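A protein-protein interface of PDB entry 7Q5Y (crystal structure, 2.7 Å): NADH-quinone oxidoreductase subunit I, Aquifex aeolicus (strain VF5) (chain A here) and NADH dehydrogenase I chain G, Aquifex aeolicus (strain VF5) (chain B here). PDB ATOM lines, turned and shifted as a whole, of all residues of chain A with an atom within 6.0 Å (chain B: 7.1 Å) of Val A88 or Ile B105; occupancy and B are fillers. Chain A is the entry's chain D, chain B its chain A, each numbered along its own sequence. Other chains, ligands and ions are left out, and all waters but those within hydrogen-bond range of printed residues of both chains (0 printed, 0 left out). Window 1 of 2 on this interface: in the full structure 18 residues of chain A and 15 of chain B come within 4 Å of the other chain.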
ATOM      1  N   LEU A  71       2.824  -7.738  -3.534  1.00  0.00           N
ATOM      2  CA  LEU A  71       3.438  -8.909  -2.906  1.00  0.00           C
ATOM      3  C   LEU A  71       3.826  -9.946  -3.952  1.00  0.00           C
ATOM      4  O   LEU A  71       4.951 -10.463  -3.933  1.00  0.00           O
ATOM      5  CB  LEU A  71       2.512  -9.540  -1.859  1.00  0.00           C
ATOM      6  CG  LEU A  71       3.018 -10.863  -1.225  1.00  0.00           C
ATOM      7  CD1 LEU A  71       4.415 -10.723  -0.684  1.00  0.00           C
ATOM      8  CD2 LEU A  71       2.128 -11.408  -0.120  1.00  0.00           C
ATOM      9  N   ILE A  74       7.134  -9.457  -5.470  1.00  0.00           N
ATOM     10  CA  ILE A  74       8.341  -9.767  -4.711  1.00  0.00           C
ATOM     11  C   ILE A  74       8.331 -11.192  -4.186  1.00  0.00           C
ATOM     12  O   ILE A  74       9.237 -11.578  -3.443  1.00  0.00           O
ATOM     13  CB  ILE A  74       8.576  -8.791  -3.543  1.00  0.00           C
ATOM     14  CG1 ILE A  74       7.522  -8.960  -2.464  1.00  0.00           C
ATOM     15  CG2 ILE A  74       8.613  -7.371  -3.998  1.00  0.00           C
ATOM     16  CD1 ILE A  74       7.736  -7.971  -1.336  1.00  0.00           C
ATOM     17  N   PHE A  77      11.462 -13.373  -4.137  1.00  0.00           N
ATOM     18  CA  PHE A  77      12.501 -13.145  -3.148  1.00  0.00           C
ATOM     19  C   PHE A  77      12.204 -13.756  -1.791  1.00  0.00           C
ATOM     20  O   PHE A  77      13.093 -13.774  -0.931  1.00  0.00           O
ATOM     21  CB  PHE A  77      12.719 -11.654  -2.925  1.00  0.00           C
ATOM     22  CG  PHE A  77      13.008 -10.889  -4.177  1.00  0.00           C
ATOM     23  CD1 PHE A  77      14.121 -11.172  -4.931  1.00  0.00           C
ATOM     24  CD2 PHE A  77      12.202  -9.842  -4.558  1.00  0.00           C
ATOM     25  CE1 PHE A  77      14.393 -10.463  -6.063  1.00  0.00           C
ATOM     26  CE2 PHE A  77      12.481  -9.128  -5.683  1.00  0.00           C
ATOM     27  CZ  PHE A  77      13.571  -9.445  -6.440  1.00  0.00           C
ATOM     28  N   MET A  78      10.987 -14.227  -1.565  1.00  0.00           N
ATOM     29  CA  MET A  78      10.581 -14.726  -0.263  1.00  0.00           C
ATOM     30  C   MET A  78      10.586 -16.238  -0.076  1.00  0.00           C
ATOM     31  O   MET A  78      10.401 -17.024  -1.011  1.00  0.00           O
ATOM     32  CB  MET A  78       9.184 -14.214   0.044  1.00  0.00           C
ATOM     33  CG  MET A  78       9.088 -12.699   0.071  1.00  0.00           C
ATOM     34  SD  MET A  78       9.937 -12.045   1.505  1.00  0.00           S
ATOM     35  CE  MET A  78      11.370 -11.362   0.718  1.00  0.00           C
ATOM     36  N   ARG A  86       2.062 -13.672   5.200  1.00  0.00           N
ATOM     37  CA  ARG A  86       2.527 -12.982   4.010  1.00  0.00           C
ATOM     38  C   ARG A  86       3.663 -12.017   4.293  1.00  0.00           C
ATOM     39  O   ARG A  86       4.339 -11.594   3.345  1.00  0.00           O
ATOM     40  CB  ARG A  86       1.392 -12.155   3.402  1.00  0.00           C
ATOM     41  CG  ARG A  86       0.220 -12.919   2.831  1.00  0.00           C
ATOM     42  CD  ARG A  86      -0.884 -11.939   2.479  1.00  0.00           C
ATOM     43  NE  ARG A  86      -1.870 -12.516   1.572  1.00  0.00           N
ATOM     44  CZ  ARG A  86      -2.984 -11.895   1.198  1.00  0.00           C
ATOM     45  NH1 ARG A  86      -3.822 -12.485   0.362  1.00  0.00           N
ATOM     46  NH2 ARG A  86      -3.260 -10.682   1.663  1.00  0.00           N
ATOM     47  N   CYS A  87       3.841 -11.633   5.559  1.00  0.00           N
ATOM     48  CA  CYS A  87       4.844 -10.652   5.962  1.00  0.00           C
ATOM     49  C   CYS A  87       6.215 -10.919   5.345  1.00  0.00           C
ATOM     50  O   CYS A  87       6.686 -12.059   5.306  1.00  0.00           O
ATOM     51  CB  CYS A  87       4.930 -10.609   7.495  1.00  0.00           C
ATOM     52  SG  CYS A  87       6.084  -9.422   8.230  1.00  0.00           S
ATOM     53  N   VAL A  88       6.836  -9.832   4.868  1.00  0.00           N
ATOM     54  CA  VAL A  88       8.158  -9.775   4.257  1.00  0.00           C
ATOM     55  C   VAL A  88       9.119  -8.961   5.114  1.00  0.00           C
ATOM     56  O   VAL A  88      10.229  -8.665   4.675  1.00  0.00           O
ATOM     57  CB  VAL A  88       8.123  -9.197   2.819  1.00  0.00           C
ATOM     58  CG1 VAL A  88       7.123  -9.913   1.905  1.00  0.00           C
ATOM     59  CG2 VAL A  88       7.795  -7.717   2.846  1.00  0.00           C
ATOM     60  N   ALA A  89       8.719  -8.606   6.338  1.00  0.00           N
ATOM     61  CA  ALA A  89       9.543  -7.861   7.294  1.00  0.00           C
ATOM     62  C   ALA A  89      10.116  -6.573   6.708  1.00  0.00           C
ATOM     63  O   ALA A  89      11.329  -6.396   6.594  1.00  0.00           O
ATOM     64  CB  ALA A  89      10.672  -8.734   7.823  1.00  0.00           C
ATOM     65  N   CYS A  90       9.222  -5.674   6.327  1.00  0.00           N
ATOM     66  CA  CYS A  90       9.635  -4.394   5.766  1.00  0.00           C
ATOM     67  C   CYS A  90       9.786  -3.307   6.825  1.00  0.00           C
ATOM     68  O   CYS A  90      10.406  -2.270   6.553  1.00  0.00           O
ATOM     69  CB  CYS A  90       8.640  -3.975   4.682  1.00  0.00           C
ATOM     70  SG  CYS A  90       6.990  -3.392   5.211  1.00  0.00           S
ATOM     71  N   ALA A 107      13.917 -10.908  10.724  1.00  0.00           N
ATOM     72  CA  ALA A 107      13.986 -11.627   9.465  1.00  0.00           C
ATOM     73  C   ALA A 107      15.434 -11.977   9.210  1.00  0.00           C
ATOM     74  O   ALA A 107      16.349 -11.342   9.737  1.00  0.00           O
ATOM     75  CB  ALA A 107      13.454 -10.815   8.283  1.00  0.00           C
ATOM     76  N   LYS A 115      14.599 -14.328   1.543  1.00  0.00           N
ATOM     77  CA  LYS A 115      14.360 -13.687   2.825  1.00  0.00           C
ATOM     78  C   LYS A 115      13.258 -14.452   3.547  1.00  0.00           C
ATOM     79  O   LYS A 115      12.302 -14.911   2.920  1.00  0.00           O
ATOM     80  CB  LYS A 115      13.981 -12.212   2.646  1.00  0.00           C
ATOM     81  CG  LYS A 115      13.503 -11.487   3.919  1.00  0.00           C
ATOM     82  CD  LYS A 115      13.323  -9.967   3.715  1.00  0.00           C
ATOM     83  CE  LYS A 115      13.086  -9.294   5.050  1.00  0.00           C
ATOM     84  NZ  LYS A 115      13.060  -7.814   5.121  1.00  0.00           N
ATOM     85  N   VAL A 117      10.903 -14.426   7.271  1.00  0.00           N
ATOM     86  CA  VAL A 117      10.520 -13.763   8.508  1.00  0.00           C
ATOM     87  C   VAL A 117      10.558 -14.811   9.609  1.00  0.00           C
ATOM     88  O   VAL A 117       9.964 -15.892   9.488  1.00  0.00           O
ATOM     89  CB  VAL A 117       9.138 -13.109   8.380  1.00  0.00           C
ATOM     90  CG1 VAL A 117       8.696 -12.574   9.716  1.00  0.00           C
ATOM     91  CG2 VAL A 117       9.199 -11.985   7.375  1.00  0.00           C
ATOM     92  N   PRO A 138       2.523  -2.528   2.923  1.00  0.00           N
ATOM     93  CA  PRO A 138       2.516  -2.484   1.455  1.00  0.00           C
ATOM     94  C   PRO A 138       2.262  -3.810   0.756  1.00  0.00           C
ATOM     95  O   PRO A 138       2.218  -3.843  -0.476  1.00  0.00           O
ATOM     96  CB  PRO A 138       3.936  -1.992   1.169  1.00  0.00           C
ATOM     97  CG  PRO A 138       4.765  -2.724   2.253  1.00  0.00           C
ATOM     98  CD  PRO A 138       3.872  -2.799   3.468  1.00  0.00           C
ATOM     99  N   VAL A 139       2.097  -4.887   1.511  1.00  0.00           N
ATOM    100  CA  VAL A 139       1.932  -6.231   0.985  1.00  0.00           C
ATOM    101  C   VAL A 139       0.574  -6.849   1.336  1.00  0.00           C
ATOM    102  O   VAL A 139       0.268  -7.966   0.892  1.00  0.00           O
ATOM    103  CB  VAL A 139       3.129  -7.081   1.486  1.00  0.00           C
ATOM    104  CG1 VAL A 139       2.853  -8.546   1.700  1.00  0.00           C
ATOM    105  CG2 VAL A 139       4.298  -6.895   0.544  1.00  0.00           C
ATOM    106  N   CYS A 141      -0.627  -7.666   4.430  1.00  0.00           N
ATOM    107  CA  CYS A 141      -0.417  -8.662   5.469  1.00  0.00           C
ATOM    108  C   CYS A 141      -1.020  -8.231   6.798  1.00  0.00           C
ATOM    109  O   CYS A 141      -1.877  -8.937   7.334  1.00  0.00           O
ATOM    110  CB  CYS A 141       1.091  -8.935   5.640  1.00  0.00           C
ATOM    111  SG  CYS A 141       1.541  -9.971   7.094  1.00  0.00           S
ATOM    112  N   LEU B 101       8.134  -2.972  -7.802  1.00  0.00           N
ATOM    113  CA  LEU B 101       7.520  -2.640  -6.525  1.00  0.00           C
ATOM    114  C   LEU B 101       8.296  -3.386  -5.444  1.00  0.00           C
ATOM    115  O   LEU B 101       7.733  -4.117  -4.638  1.00  0.00           O
ATOM    116  CB  LEU B 101       6.051  -3.049  -6.508  1.00  0.00           C
ATOM    117  CG  LEU B 101       4.858  -2.279  -7.093  1.00  0.00           C
ATOM    118  CD1 LEU B 101       4.338  -1.287  -6.101  1.00  0.00           C
ATOM    119  CD2 LEU B 101       5.261  -1.582  -8.385  1.00  0.00           C
ATOM    120  N   ASP B 102       9.621  -3.213  -5.444  1.00  0.00           N
ATOM    121  CA  ASP B 102      10.501  -3.936  -4.542  1.00  0.00           C
ATOM    122  C   ASP B 102      10.818  -3.218  -3.236  1.00  0.00           C
ATOM    123  O   ASP B 102      11.564  -3.785  -2.416  1.00  0.00           O
ATOM    124  CB  ASP B 102      11.828  -4.281  -5.255  1.00  0.00           C
ATOM    125  CG  ASP B 102      11.710  -5.434  -6.288  1.00  0.00           C
ATOM    126  OD1 ASP B 102      10.625  -6.049  -6.452  1.00  0.00           O
ATOM    127  OD2 ASP B 102      12.750  -5.744  -6.924  1.00  0.00           O
ATOM    128  N   CYS B 103      10.295  -2.009  -3.009  1.00  0.00           N
ATOM    129  CA  CYS B 103      10.629  -1.306  -1.771  1.00  0.00           C
ATOM    130  C   CYS B 103      10.472  -2.136  -0.489  1.00  0.00           C
ATOM    131  O   CYS B 103      11.341  -2.025   0.393  1.00  0.00           O
ATOM    132  CB  CYS B 103       9.817  -0.008  -1.679  1.00  0.00           C
ATOM    133  SG  CYS B 103      10.199   1.182  -2.982  1.00  0.00           S
ATOM    134  N   PRO B 104       9.435  -2.957  -0.305  1.00  0.00           N
ATOM    135  CA  PRO B 104       9.347  -3.697   0.957  1.00  0.00           C
ATOM    136  C   PRO B 104      10.547  -4.550   1.264  1.00  0.00           C
ATOM    137  O   PRO B 104      10.847  -4.762   2.439  1.00  0.00           O
ATOM    138  CB  PRO B 104       8.091  -4.555   0.766  1.00  0.00           C
ATOM    139  CG  PRO B 104       7.252  -3.767  -0.128  1.00  0.00           C
ATOM    140  CD  PRO B 104       8.205  -3.124  -1.101  1.00  0.00           C
ATOM    141  N   ILE B 105      11.266  -5.053   0.267  1.00  0.00           N
ATOM    142  CA  ILE B 105      12.400  -5.918   0.558  1.00  0.00           C
ATOM    143  C   ILE B 105      13.722  -5.385   0.037  1.00  0.00           C
ATOM    144  O   ILE B 105      14.738  -6.049   0.198  1.00  0.00           O
ATOM    145  CB  ILE B 105      12.148  -7.346   0.038  1.00  0.00           C
ATOM    146  CG1 ILE B 105      11.865  -7.349  -1.450  1.00  0.00           C
ATOM    147  CG2 ILE B 105      10.924  -7.898   0.713  1.00  0.00           C
ATOM    148  CD1 ILE B 105      13.081  -7.394  -2.310  1.00  0.00           C
ATOM    149  N   CYS B 106      13.731  -4.225  -0.599  1.00  0.00           N
ATOM    150  CA  CYS B 106      14.947  -3.649  -1.156  1.00  0.00           C
ATOM    151  C   CYS B 106      15.815  -3.020  -0.066  1.00  0.00           C
ATOM    152  O   CYS B 106      15.311  -2.317   0.812  1.00  0.00           O
ATOM    153  CB  CYS B 106      14.553  -2.630  -2.224  1.00  0.00           C
ATOM    154  SG  CYS B 106      15.826  -1.629  -2.938  1.00  0.00           S
ATOM    155  N   ASP B 107      17.128  -3.291  -0.113  1.00  0.00           N
ATOM    156  CA  ASP B 107      18.047  -2.779   0.907  1.00  0.00           C
ATOM    157  C   ASP B 107      18.213  -1.272   0.892  1.00  0.00           C
ATOM    158  O   ASP B 107      18.685  -0.711   1.883  1.00  0.00           O
ATOM    159  CB  ASP B 107      19.458  -3.374   0.765  1.00  0.00           C
ATOM    160  CG  ASP B 107      19.524  -4.864   1.056  1.00  0.00           C
ATOM    161  OD1 ASP B 107      18.696  -5.362   1.860  1.00  0.00           O
ATOM    162  OD2 ASP B 107      20.462  -5.513   0.520  1.00  0.00           O
ATOM    163  N   LYS B 108      17.862  -0.604  -0.197  1.00  0.00           N
ATOM    164  CA  LYS B 108      18.045   0.838  -0.291  1.00  0.00           C
ATOM    165  C   LYS B 108      16.891   1.655   0.291  1.00  0.00           C
ATOM    166  O   LYS B 108      17.058   2.874   0.463  1.00  0.00           O
ATOM    167  CB  LYS B 108      18.254   1.227  -1.762  1.00  0.00           C
ATOM    168  CG  LYS B 108      19.120   2.478  -1.955  1.00  0.00           C
ATOM    169  CD  LYS B 108      20.559   2.082  -2.141  1.00  0.00           C
ATOM    170  CE  LYS B 108      21.472   3.235  -2.357  1.00  0.00           C
ATOM    171  NZ  LYS B 108      22.867   2.687  -2.623  1.00  0.00           N
ATOM    172  N   ALA B 109      15.748   1.029   0.600  1.00  0.00           N
ATOM    173  CA  ALA B 109      14.596   1.761   1.121  1.00  0.00           C
ATOM    174  C   ALA B 109      14.988   2.672   2.275  1.00  0.00           C
ATOM    175  O   ALA B 109      15.676   2.254   3.203  1.00  0.00           O
ATOM    176  CB  ALA B 109      13.514   0.781   1.562  1.00  0.00           C
ATOM    177  N   TYR B 150      20.329  -5.719  -9.922  1.00  0.00           N
ATOM    178  CA  TYR B 150      18.892  -5.738 -10.185  1.00  0.00           C
ATOM    179  C   TYR B 150      18.715  -4.683 -11.285  1.00  0.00           C
ATOM    180  O   TYR B 150      18.587  -3.488 -11.006  1.00  0.00           O
ATOM    181  CB  TYR B 150      18.084  -5.437  -8.905  1.00  0.00           C
ATOM    182  CG  TYR B 150      18.220  -6.468  -7.793  1.00  0.00           C
ATOM    183  CD1 TYR B 150      19.399  -6.575  -7.044  1.00  0.00           C
ATOM    184  CD2 TYR B 150      17.155  -7.291  -7.446  1.00  0.00           C
ATOM    185  CE1 TYR B 150      19.522  -7.493  -6.011  1.00  0.00           C
ATOM    186  CE2 TYR B 150      17.262  -8.229  -6.423  1.00  0.00           C
ATOM    187  CZ  TYR B 150      18.444  -8.325  -5.710  1.00  0.00           C
ATOM    188  OH  TYR B 150      18.525  -9.244  -4.703  1.00  0.00           O
ATOM    189  N   ARG B 153      15.820  -2.206 -11.292  1.00  0.00           N
ATOM    190  CA  ARG B 153      15.908  -1.130 -10.327  1.00  0.00           C
ATOM    191  C   ARG B 153      16.887  -0.087 -10.818  1.00  0.00           C
ATOM    192  O   ARG B 153      16.886   1.043 -10.318  1.00  0.00           O
ATOM    193  CB  ARG B 153      16.360  -1.649  -8.944  1.00  0.00           C
ATOM    194  CG  ARG B 153      15.628  -2.891  -8.406  1.00  0.00           C
ATOM    195  CD  ARG B 153      15.428  -2.821  -6.873  1.00  0.00           C
ATOM    196  NE  ARG B 153      16.449  -3.558  -6.127  1.00  0.00           N
ATOM    197  CZ  ARG B 153      16.262  -4.655  -5.393  1.00  0.00           C
ATOM    198  NH1 ARG B 153      15.079  -5.227  -5.233  1.00  0.00           N
ATOM    199  NH2 ARG B 153      17.300  -5.182  -4.799  1.00  0.00           N
ATOM    200  N   LYS B 217      22.104  -7.968   2.515  1.00  0.00           N
ATOM    201  CA  LYS B 217      20.751  -8.230   2.031  1.00  0.00           C
ATOM    202  C   LYS B 217      19.810  -8.865   3.065  1.00  0.00           C
ATOM    203  O   LYS B 217      20.107  -9.904   3.662  1.00  0.00           O
ATOM    204  CB  LYS B 217      20.845  -9.111   0.780  1.00  0.00           C
ATOM    205  CG  LYS B 217      19.618  -9.126  -0.104  1.00  0.00           C
ATOM    206  CD  LYS B 217      19.869  -9.823  -1.453  1.00  0.00           C
ATOM    207  CE  LYS B 217      20.081 -11.307  -1.277  1.00  0.00           C
ATOM    208  NZ  LYS B 217      19.977 -12.111  -2.538  1.00  0.00           N
ATOM    209  N   TYR B 218      18.668  -8.204   3.267  1.00  0.00           N
ATOM    210  CA  TYR B 218      17.552  -8.610   4.115  1.00  0.00           C
ATOM    211  C   TYR B 218      17.838  -8.672   5.608  1.00  0.00           C
ATOM    212  O   TYR B 218      16.950  -9.014   6.393  1.00  0.00           O
ATOM    213  CB  TYR B 218      17.008  -9.966   3.651  1.00  0.00           C
ATOM    214  CG  TYR B 218      16.722 -10.097   2.164  1.00  0.00           C
ATOM    215  CD1 TYR B 218      16.093  -9.088   1.457  1.00  0.00           C
ATOM    216  CD2 TYR B 218      17.075 -11.242   1.478  1.00  0.00           C
ATOM    217  CE1 TYR B 218      15.830  -9.225   0.093  1.00  0.00           C
ATOM    218  CE2 TYR B 218      16.810 -11.392   0.145  1.00  0.00           C
ATOM    219  CZ  TYR B 218      16.198 -10.382  -0.553  1.00  0.00           C
ATOM    220  OH  TYR B 218      15.957 -10.552  -1.899  1.00  0.00           O
ATOM    221  N   SER B 220      18.476  -6.159   7.630  1.00  0.00           N
ATOM    222  CA  SER B 220      17.927  -5.031   8.368  1.00  0.00           C
ATOM    223  C   SER B 220      17.288  -4.063   7.371  1.00  0.00           C
ATOM    224  O   SER B 220      16.969  -4.439   6.239  1.00  0.00           O
ATOM    225  CB  SER B 220      19.046  -4.389   9.207  1.00  0.00           C
ATOM    226  OG  SER B 220      18.542  -3.447  10.132  1.00  0.00           O
ATOM    227  N   ARG B 221      17.076  -2.831   7.809  1.00  0.00           N
ATOM    228  CA  ARG B 221      16.551  -1.736   7.012  1.00  0.00           C
ATOM    229  C   ARG B 221      17.482  -0.567   7.296  1.00  0.00           C
ATOM    230  O   ARG B 221      17.942  -0.389   8.428  1.00  0.00           O
ATOM    231  CB  ARG B 221      15.099  -1.362   7.341  1.00  0.00           C
ATOM    232  CG  ARG B 221      14.164  -2.537   7.338  1.00  0.00           C
ATOM    233  CD  ARG B 221      14.002  -3.075   5.938  1.00  0.00           C
ATOM    234  NE  ARG B 221      12.932  -2.435   5.201  1.00  0.00           N
ATOM    235  CZ  ARG B 221      12.902  -2.379   3.879  1.00  0.00           C
ATOM    236  NH1 ARG B 221      13.905  -2.902   3.200  1.00  0.00           N
ATOM    237  NH2 ARG B 221      11.893  -1.784   3.247  1.00  0.00           N
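OD1 of Asp B107 is in hydrogen-bond range of N of Tyr B218 (3.2 Å).
The guanidinium group of Arg B221 lies within hydrogen-bond range of the backbone carbonyl oxygen of Pro B104 (3.3 Å).
The backbone carbonyl oxygen of Cys B106 lies within hydrogen-bond range of the guanidinium group of Arg B221, at 2.8 Å.
NH2 of Arg B221 lies within hydrogen-bond range of O of Cys B103 (2.9 Å).
O of Val A88 sits close to NZ of Lys A115.
The backbone NH (N) of Lys A115 sits at hydrogen-bond distance from the backbone carbonyl oxygen (O) of Phe A77, at 2.9 Å.
Among the printed residues, merely in contact across the chains: Ile A74 with Leu B101 (3.4 Å), Ile A74 with Asp B102 (3.4 Å), Ile A74 with Ile B105 (3.8 Å), Phe A77 with Asp B102 (3.6 Å), Phe A77 with Ile B105 (3.4 Å), Phe A77 with Tyr B150 (3.7 Å), Phe A77 with Tyr B218 (3.6 Å), Met A78 with Ile B105 (3.5 Å), Val A88 with Pro B104 (3.8 Å), Val A88 with Ile B105 (3.7 Å), Cys A90 with Pro B104 (3.2 Å), Lys A115 with Tyr B218 (3.4 Å) and Pro A138 with Pro B104 (3.6 Å).
Of the 15 printed residues of chain B, 7 touch a printed residue of chain A.
Along chain B the printed residues that touch a printed residue of chain A span positions 101 to 221.
Among the printed residues, 14 pairs touch across the chains.
The backbone carbonyl oxygen (O) of Cys A90 lies within hydrogen-bond range of the guanidinium group (NE) of Arg B221.
Val A88 touches just these residues of chain B: Pro B104 and Ile B105.
Val A117 touches none of the printed residues of chain B.
Cys A141 touches none of the printed residues of chain B.
Of the printed residues of chain A, Leu B101 touches Ile A74 (3.4 Å).
Of chain A, only Ile A74, Phe A77, Met A78 and Val A88 come within 4 Å of Ile B105.
Of the printed residues of chain A, Tyr B218 touches Phe A77 (3.6 Å) and Lys A115 (3.4 Å).
The nearest residue of chain A that does not touch Ile B105 is Lys A115 (4.4 Å).
The nearest printed residue of chain B that does not touch Ile A74 is Pro B104 (4.03 Å).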
